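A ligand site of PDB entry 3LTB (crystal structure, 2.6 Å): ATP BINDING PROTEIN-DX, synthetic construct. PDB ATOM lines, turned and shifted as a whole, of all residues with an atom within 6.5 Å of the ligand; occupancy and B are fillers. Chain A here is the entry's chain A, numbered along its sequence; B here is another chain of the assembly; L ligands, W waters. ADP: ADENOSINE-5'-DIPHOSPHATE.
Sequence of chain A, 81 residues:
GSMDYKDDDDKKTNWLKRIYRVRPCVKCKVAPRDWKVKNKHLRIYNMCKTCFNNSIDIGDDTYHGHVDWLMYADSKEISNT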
ATOM      1  N   ARG A  33       0.345   9.098 -18.100  1.00  0.00           N
ATOM      2  CA  ARG A  33       0.972   8.187 -17.159  1.00  0.00           C
ATOM      3  C   ARG A  33       0.689   6.691 -17.452  1.00  0.00           C
ATOM      4  O   ARG A  33      -0.366   6.301 -18.025  1.00  0.00           O
ATOM      5  CB  ARG A  33       0.499   8.520 -15.744  1.00  0.00           C
ATOM      6  CG  ARG A  33       0.917   9.862 -15.252  1.00  0.00           C
ATOM      7  CD  ARG A  33       0.211  10.261 -13.944  1.00  0.00           C
ATOM      8  NE  ARG A  33       0.528  11.642 -13.648  1.00  0.00           N
ATOM      9  CZ  ARG A  33       0.540  12.179 -12.431  1.00  0.00           C
ATOM     10  NH1 ARG A  33       0.244  11.436 -11.353  1.00  0.00           N
ATOM     11  NH2 ARG A  33       0.866  13.462 -12.306  1.00  0.00           N
ATOM     12  N   ASP A  34       1.610   5.845 -17.009  1.00  0.00           N
ATOM     13  CA  ASP A  34       1.365   4.431 -16.978  1.00  0.00           C
ATOM     14  C   ASP A  34       0.290   4.166 -15.921  1.00  0.00           C
ATOM     15  O   ASP A  34       0.040   5.006 -15.071  1.00  0.00           O
ATOM     16  CB  ASP A  34       2.648   3.666 -16.624  1.00  0.00           C
ATOM     17  CG  ASP A  34       2.526   2.178 -16.929  1.00  0.00           C
ATOM     18  OD1 ASP A  34       1.585   1.802 -17.644  1.00  0.00           O
ATOM     19  OD2 ASP A  34       3.354   1.384 -16.456  1.00  0.00           O
ATOM     20  N   TRP A  35      -0.337   3.002 -15.982  1.00  0.00           N
ATOM     21  CA  TRP A  35      -1.407   2.631 -15.064  1.00  0.00           C
ATOM     22  C   TRP A  35      -1.621   1.140 -15.169  1.00  0.00           C
ATOM     23  O   TRP A  35      -1.172   0.495 -16.115  1.00  0.00           O
ATOM     24  CB  TRP A  35      -2.696   3.306 -15.484  1.00  0.00           C
ATOM     25  CG  TRP A  35      -3.064   2.972 -16.895  1.00  0.00           C
ATOM     26  CD1 TRP A  35      -2.596   3.587 -18.019  1.00  0.00           C
ATOM     27  CD2 TRP A  35      -4.006   1.980 -17.348  1.00  0.00           C
ATOM     28  NE1 TRP A  35      -3.171   3.046 -19.130  1.00  0.00           N
ATOM     29  CE2 TRP A  35      -4.031   2.043 -18.753  1.00  0.00           C
ATOM     30  CE3 TRP A  35      -4.816   1.037 -16.698  1.00  0.00           C
ATOM     31  CZ2 TRP A  35      -4.861   1.201 -19.539  1.00  0.00           C
ATOM     32  CZ3 TRP A  35      -5.624   0.193 -17.459  1.00  0.00           C
ATOM     33  CH2 TRP A  35      -5.650   0.285 -18.876  1.00  0.00           C
ATOM     34  N   LYS A  36      -2.334   0.572 -14.206  1.00  0.00           N
ATOM     35  CA  LYS A  36      -2.799  -0.797 -14.334  1.00  0.00           C
ATOM     36  C   LYS A  36      -4.076  -0.981 -13.527  1.00  0.00           C
ATOM     37  O   LYS A  36      -4.403  -0.169 -12.653  1.00  0.00           O
ATOM     38  CB  LYS A  36      -1.704  -1.825 -13.971  1.00  0.00           C
ATOM     39  CG  LYS A  36      -1.542  -2.096 -12.508  1.00  0.00           C
ATOM     40  CD  LYS A  36      -0.533  -3.225 -12.210  1.00  0.00           C
ATOM     41  CE  LYS A  36      -0.704  -3.692 -10.749  1.00  0.00           C
ATOM     42  NZ  LYS A  36       0.577  -4.081 -10.034  1.00  0.00           N
ATOM     43  N   LYS A  38      -6.114  -3.107 -10.874  1.00  0.00           N
ATOM     44  CA  LYS A  38      -5.647  -3.804  -9.669  1.00  0.00           C
ATOM     45  C   LYS A  38      -6.898  -4.187  -8.844  1.00  0.00           C
ATOM     46  O   LYS A  38      -7.301  -3.442  -7.947  1.00  0.00           O
ATOM     47  CB  LYS A  38      -4.731  -2.828  -8.897  1.00  0.00           C
ATOM     48  CG  LYS A  38      -4.224  -3.259  -7.509  1.00  0.00           C
ATOM     49  CD  LYS A  38      -2.718  -3.558  -7.492  1.00  0.00           C
ATOM     50  CE  LYS A  38      -2.354  -4.402  -6.260  1.00  0.00           C
ATOM     51  NZ  LYS A  38      -0.930  -4.828  -6.283  1.00  0.00           N
ATOM     52  N   ARG A  43      -4.750   1.898 -10.655  1.00  0.00           N
ATOM     53  CA  ARG A  43      -3.500   2.463 -10.160  1.00  0.00           C
ATOM     54  C   ARG A  43      -2.938   3.396 -11.240  1.00  0.00           C
ATOM     55  O   ARG A  43      -2.610   2.934 -12.340  1.00  0.00           O
ATOM     56  CB  ARG A  43      -2.508   1.330  -9.872  1.00  0.00           C
ATOM     57  CG  ARG A  43      -1.111   1.776  -9.482  1.00  0.00           C
ATOM     58  CD  ARG A  43      -0.351   0.656  -8.785  1.00  0.00           C
ATOM     59  NE  ARG A  43      -0.921   0.460  -7.459  1.00  0.00           N
ATOM     60  CZ  ARG A  43      -0.424  -0.339  -6.518  1.00  0.00           C
ATOM     61  NH1 ARG A  43       0.677  -1.039  -6.726  1.00  0.00           N
ATOM     62  NH2 ARG A  43      -1.027  -0.413  -5.345  1.00  0.00           N
ATOM     63  N   TYR A  45       0.252   5.442 -12.132  1.00  0.00           N
ATOM     64  CA  TYR A  45       1.653   5.658 -11.773  1.00  0.00           C
ATOM     65  C   TYR A  45       2.019   7.098 -12.045  1.00  0.00           C
ATOM     66  O   TYR A  45       1.436   7.735 -12.938  1.00  0.00           O
ATOM     67  CB  TYR A  45       2.551   4.744 -12.589  1.00  0.00           C
ATOM     68  CG  TYR A  45       2.336   3.283 -12.279  1.00  0.00           C
ATOM     69  CD1 TYR A  45       2.702   2.762 -11.032  1.00  0.00           C
ATOM     70  CD2 TYR A  45       1.804   2.428 -13.218  1.00  0.00           C
ATOM     71  CE1 TYR A  45       2.521   1.443 -10.730  1.00  0.00           C
ATOM     72  CE2 TYR A  45       1.609   1.094 -12.925  1.00  0.00           C
ATOM     73  CZ  TYR A  45       1.973   0.614 -11.677  1.00  0.00           C
ATOM     74  OH  TYR A  45       1.800  -0.703 -11.371  1.00  0.00           O
ATOM     75  N   ASN A  46       2.959   7.633 -11.289  1.00  0.00           N
ATOM     76  CA  ASN A  46       3.358   9.024 -11.510  1.00  0.00           C
ATOM     77  C   ASN A  46       4.026   9.314 -12.867  1.00  0.00           C
ATOM     78  O   ASN A  46       3.983  10.444 -13.363  1.00  0.00           O
ATOM     79  CB  ASN A  46       4.293   9.491 -10.380  1.00  0.00           C
ATOM     80  CG  ASN A  46       3.717   9.262  -9.048  1.00  0.00           C
ATOM     81  OD1 ASN A  46       2.509   9.430  -8.831  1.00  0.00           O
ATOM     82  ND2 ASN A  46       4.562   8.872  -8.098  1.00  0.00           N
ATOM     83  N   MET A  47       4.676   8.299 -13.450  1.00  0.00           N
ATOM     84  CA  MET A  47       5.386   8.495 -14.707  1.00  0.00           C
ATOM     85  C   MET A  47       4.821   7.650 -15.883  1.00  0.00           C
ATOM     86  O   MET A  47       4.214   6.590 -15.664  1.00  0.00           O
ATOM     87  CB  MET A  47       6.865   8.169 -14.487  1.00  0.00           C
ATOM     88  CG  MET A  47       7.658   9.289 -13.826  1.00  0.00           C
ATOM     89  SD  MET A  47       9.439   8.897 -13.656  1.00  0.00           S
ATOM     90  CE  MET A  47       9.368   7.504 -12.499  1.00  0.00           C
ATOM     91  N   CYS A  48       5.041   8.120 -17.121  1.00  0.00           N
ATOM     92  CA  CYS A  48       4.792   7.269 -18.301  1.00  0.00           C
ATOM     93  C   CYS A  48       5.813   6.140 -18.250  1.00  0.00           C
ATOM     94  O   CYS A  48       6.723   6.177 -17.429  1.00  0.00           O
ATOM     95  CB  CYS A  48       4.911   8.047 -19.629  1.00  0.00           C
ATOM     96  SG  CYS A  48       6.556   8.744 -19.940  1.00  0.00           S
ATOM     97  N   LYS A  49       5.686   5.124 -19.103  1.00  0.00           N
ATOM     98  CA  LYS A  49       6.622   4.005 -19.054  1.00  0.00           C
ATOM     99  C   LYS A  49       8.035   4.416 -19.475  1.00  0.00           C
ATOM    100  O   LYS A  49       9.016   3.928 -18.912  1.00  0.00           O
ATOM    101  CB  LYS A  49       6.149   2.849 -19.938  1.00  0.00           C
ATOM    102  CG  LYS A  49       6.799   1.502 -19.589  1.00  0.00           C
ATOM    103  CD  LYS A  49       6.032   0.757 -18.503  1.00  0.00           C
ATOM    104  CE  LYS A  49       6.955  -0.186 -17.786  1.00  0.00           C
ATOM    105  NZ  LYS A  49       6.367  -0.808 -16.535  1.00  0.00           N
ATOM    106  N   CYS A  51       9.629   7.196 -19.104  1.00  0.00           N
ATOM    107  CA  CYS A  51      10.357   7.914 -18.059  1.00  0.00           C
ATOM    108  C   CYS A  51      10.634   7.022 -16.878  1.00  0.00           C
ATOM    109  O   CYS A  51      11.680   7.179 -16.229  1.00  0.00           O
ATOM    110  CB  CYS A  51       9.617   9.184 -17.598  1.00  0.00           C
ATOM    111  SG  CYS A  51       9.598  10.506 -18.831  1.00  0.00           S
ATOM    112  N   PHE A  52       9.696   6.106 -16.577  1.00  0.00           N
ATOM    113  CA  PHE A  52       9.925   5.118 -15.531  1.00  0.00           C
ATOM    114  C   PHE A  52      11.165   4.248 -15.806  1.00  0.00           C
ATOM    115  O   PHE A  52      12.089   4.208 -14.969  1.00  0.00           O
ATOM    116  CB  PHE A  52       8.716   4.243 -15.279  1.00  0.00           C
ATOM    117  CG  PHE A  52       8.972   3.188 -14.245  1.00  0.00           C
ATOM    118  CD1 PHE A  52       9.244   3.552 -12.910  1.00  0.00           C
ATOM    119  CD2 PHE A  52       8.962   1.815 -14.597  1.00  0.00           C
ATOM    120  CE1 PHE A  52       9.490   2.563 -11.913  1.00  0.00           C
ATOM    121  CE2 PHE A  52       9.220   0.825 -13.639  1.00  0.00           C
ATOM    122  CZ  PHE A  52       9.485   1.191 -12.274  1.00  0.00           C
ATOM    123  N   ASN A  53      11.209   3.566 -16.962  1.00  0.00           N
ATOM    124  CA  ASN A  53      12.370   2.758 -17.359  1.00  0.00           C
ATOM    125  C   ASN A  53      13.631   3.604 -17.398  1.00  0.00           C
ATOM    126  O   ASN A  53      14.704   3.174 -17.000  1.00  0.00           O
ATOM    127  CB  ASN A  53      12.161   2.115 -18.738  1.00  0.00           C
ATOM    128  CG  ASN A  53      11.069   1.007 -18.729  1.00  0.00           C
ATOM    129  OD1 ASN A  53      10.753   0.423 -17.678  1.00  0.00           O
ATOM    130  ND2 ASN A  53      10.482   0.746 -19.904  1.00  0.00           N
ATOM    131  N   TYR A  63      10.801  10.151  -8.459  1.00  0.00           N
ATOM    132  CA  TYR A  63       9.430  10.267  -8.982  1.00  0.00           C
ATOM    133  C   TYR A  63       8.670   8.961  -8.988  1.00  0.00           C
ATOM    134  O   TYR A  63       7.552   8.895  -9.479  1.00  0.00           O
ATOM    135  CB  TYR A  63       9.393  10.895 -10.394  1.00  0.00           C
ATOM    136  CG  TYR A  63       9.997  12.247 -10.372  1.00  0.00           C
ATOM    137  CD1 TYR A  63       9.272  13.319  -9.854  1.00  0.00           C
ATOM    138  CD2 TYR A  63      11.320  12.463 -10.761  1.00  0.00           C
ATOM    139  CE1 TYR A  63       9.811  14.576  -9.792  1.00  0.00           C
ATOM    140  CE2 TYR A  63      11.903  13.743 -10.685  1.00  0.00           C
ATOM    141  CZ  TYR A  63      11.130  14.790 -10.194  1.00  0.00           C
ATOM    142  OH  TYR A  63      11.632  16.074 -10.084  1.00  0.00           O
ATOM    143  N   HIS A  64       9.278   7.912  -8.455  1.00  0.00           N
ATOM    144  CA  HIS A  64       8.599   6.633  -8.286  1.00  0.00           C
ATOM    145  C   HIS A  64       7.336   6.807  -7.444  1.00  0.00           C
ATOM    146  O   HIS A  64       7.343   7.565  -6.497  1.00  0.00           O
ATOM    147  CB  HIS A  64       9.570   5.642  -7.647  1.00  0.00           C
ATOM    148  CG  HIS A  64      10.631   5.171  -8.582  1.00  0.00           C
ATOM    149  ND1 HIS A  64      11.472   4.123  -8.308  1.00  0.00           N
ATOM    150  CD2 HIS A  64      10.958   5.603  -9.841  1.00  0.00           C
ATOM    151  CE1 HIS A  64      12.293   3.945  -9.333  1.00  0.00           C
ATOM    152  NE2 HIS A  64      11.997   4.824 -10.271  1.00  0.00           N
ATOM    153  N   GLY A  65       6.258   6.115  -7.778  1.00  0.00           N
ATOM    154  CA  GLY A  65       5.038   6.174  -6.950  1.00  0.00           C
ATOM    155  C   GLY A  65       3.771   5.996  -7.784  1.00  0.00           C
ATOM    156  O   GLY A  65       3.864   5.755  -8.986  1.00  0.00           O
ATOM    157  N   HIS A  66       2.602   6.132  -7.144  1.00  0.00           N
ATOM    158  CA  HIS A  66       1.322   5.876  -7.793  1.00  0.00           C
ATOM    159  C   HIS A  66       0.189   6.394  -6.943  1.00  0.00           C
ATOM    160  O   HIS A  66       0.379   6.653  -5.741  1.00  0.00           O
ATOM    161  CB  HIS A  66       1.103   4.359  -8.040  1.00  0.00           C
ATOM    162  CG  HIS A  66       1.196   3.510  -6.813  1.00  0.00           C
ATOM    163  ND1 HIS A  66       2.385   2.958  -6.366  1.00  0.00           N
ATOM    164  CD2 HIS A  66       0.256   3.107  -5.915  1.00  0.00           C
ATOM    165  CE1 HIS A  66       2.170   2.258  -5.262  1.00  0.00           C
ATOM    166  NE2 HIS A  66       0.891   2.344  -4.963  1.00  0.00           N
ATOM    167  N   ASP B   8       2.845  10.889  -2.229  1.00  0.00           N
ATOM    168  CA  ASP B   8       1.673  10.411  -2.988  1.00  0.00           C
ATOM    169  C   ASP B   8       0.283  10.571  -2.288  1.00  0.00           C
ATOM    170  O   ASP B   8      -0.718  10.826  -2.964  1.00  0.00           O
ATOM    171  CB  ASP B   8       1.866   8.953  -3.458  1.00  0.00           C
ATOM    172  CG  ASP B   8       2.984   8.798  -4.474  1.00  0.00           C
ATOM    173  OD1 ASP B   8       3.357   9.738  -5.212  1.00  0.00           O
ATOM    174  OD2 ASP B   8       3.498   7.675  -4.562  1.00  0.00           O
HETATM  175  PB  ADP L   1       3.048  -4.304  -6.744  1.00  0.00           P
HETATM  176  O1B ADP L   1       2.309  -4.088  -5.428  1.00  0.00           O
HETATM  177  O2B ADP L   1       4.297  -5.170  -6.690  1.00  0.00           O
HETATM  178  O3B ADP L   1       2.095  -4.643  -7.890  1.00  0.00           O
HETATM  179  PA  ADP L   1       3.755  -2.283  -8.582  1.00  0.00           P
HETATM  180  O1A ADP L   1       2.488  -1.526  -8.858  1.00  0.00           O
HETATM  181  O2A ADP L   1       4.172  -3.401  -9.532  1.00  0.00           O
HETATM  182  O3A ADP L   1       3.742  -2.873  -7.082  1.00  0.00           O
HETATM  183  O5' ADP L   1       4.893  -1.135  -8.403  1.00  0.00           O
HETATM  184  C5' ADP L   1       6.244  -1.359  -7.975  1.00  0.00           C
HETATM  185  C4' ADP L   1       6.947  -0.056  -7.542  1.00  0.00           C
HETATM  186  O4' ADP L   1       7.453   0.704  -8.661  1.00  0.00           O
HETATM  187  C3' ADP L   1       5.990   0.921  -6.883  1.00  0.00           C
HETATM  188  O3' ADP L   1       6.779   1.787  -6.062  1.00  0.00           O
HETATM  189  C2' ADP L   1       5.475   1.725  -8.042  1.00  0.00           C
HETATM  190  O2' ADP L   1       4.998   2.984  -7.615  1.00  0.00           O
HETATM  191  C1' ADP L   1       6.735   1.937  -8.834  1.00  0.00           C
HETATM  192  N9  ADP L   1       6.400   2.190 -10.259  1.00  0.00           N
HETATM  193  C8  ADP L   1       6.112   1.241 -11.178  1.00  0.00           C
HETATM  194  N7  ADP L   1       5.843   1.791 -12.380  1.00  0.00           N
HETATM  195  C5  ADP L   1       5.942   3.133 -12.244  1.00  0.00           C
HETATM  196  C6  ADP L   1       5.803   4.295 -13.126  1.00  0.00           C
HETATM  197  N6  ADP L   1       5.460   4.153 -14.434  1.00  0.00           N
HETATM  198  N1  ADP L   1       6.020   5.508 -12.593  1.00  0.00           N
HETATM  199  C2  ADP L   1       6.354   5.708 -11.300  1.00  0.00           C
HETATM  200  N3  ADP L   1       6.496   4.688 -10.456  1.00  0.00           N
HETATM  201  C4  ADP L   1       6.309   3.402 -10.859  1.00  0.00           C
HETATM  202  O   HOH W   1       5.788   3.552  -4.363  1.00  0.00           O
HETATM  203  O   HOH W   2       5.364   1.092 -14.906  1.00  0.00           O
HETATM  204  O   HOH W   3       3.212  -6.872  -8.845  1.00  0.00           O
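NZ of Lys 36 lies within salt-bridge range of O3B of the ligand (2.7 Å). An oxygen (O2') of the ligand sits close to the backbone carbonyl oxygen (O) of Gly 65, 3.3 Å away. The side-chain amino group of Lys 38 lies within salt-bridge range of an oxygen (O3B) of the ligand, 3.4 Å away. The backbone NH (N) of Gly 65 is in hydrogen-bond range of a nitrogen (N3) of the ligand (3.0 Å). O2' of the ligand lies within hydrogen-bond range of ND1 of His 66, 2.9 Å away. The backbone carbonyl oxygen (O) of Met 47 lies within hydrogen-bond range of a nitrogen (N6) of the ligand (3.0 Å). The side-chain hydroxyl (OH) of Tyr 45 sits at hydrogen-bond distance from an oxygen (O1A) of the ligand (2.7 Å). The guanidinium group of Arg 43 is in salt-bridge range of an oxygen (O1A) of the ligand, 2.8 Å away. N of Met 47 sits at hydrogen-bond distance from N1 of the ligand, 3.2 Å away.
The backbone carbonyl oxygen (O) of Gly 65 is in hydrogen-bond range of the backbone NH (N) of Asn 46 (3.1 Å). O of Tyr 63 is in hydrogen-bond range of ND2 of Asn 46 (3.3 Å). The side-chain amino group (NZ) of Lys 49 is in salt-bridge range of the side-chain carboxylate (OD2) of Asp 34 (3.7 Å). A ring nitrogen (NE2) of His 66 sits close to the guanidinium group (NH2) of Arg 43, at 3.4 Å. The backbone carbonyl oxygen of His 64 is in hydrogen-bond range of the side-chain amide nitrogen of Asn 46 (3.5 Å). O of Met 47 is in hydrogen-bond range of N of Asp 34. The backbone carbonyl oxygen of Lys 36 lies within hydrogen-bond range of the backbone NH of Arg 43 (2.9 Å). N of His 66 lies within hydrogen-bond range of OD2 of Asp 8 of chain B.
Residues that only touch the ligand: Phe 52, His 64, Asp 34, Cys 48, Tyr 63 and Asn 46. Within 4 Å of the ligand: Asp 34, Lys 36, Lys 38, Arg 43, Tyr 45, Asn 46, Met 47, Cys 48, Phe 52, Tyr 63, His 64, Gly 65 and His 66. The nearest printed residue that does not touch the ligand is Lys 49 (4.8 Å).
Water W2 lies within hydrogen-bond range of OD2 of Asp 34 (2.6 Å), N7 of the ligand (2.7 Å) and NZ of Lys 49 (2.7 Å).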
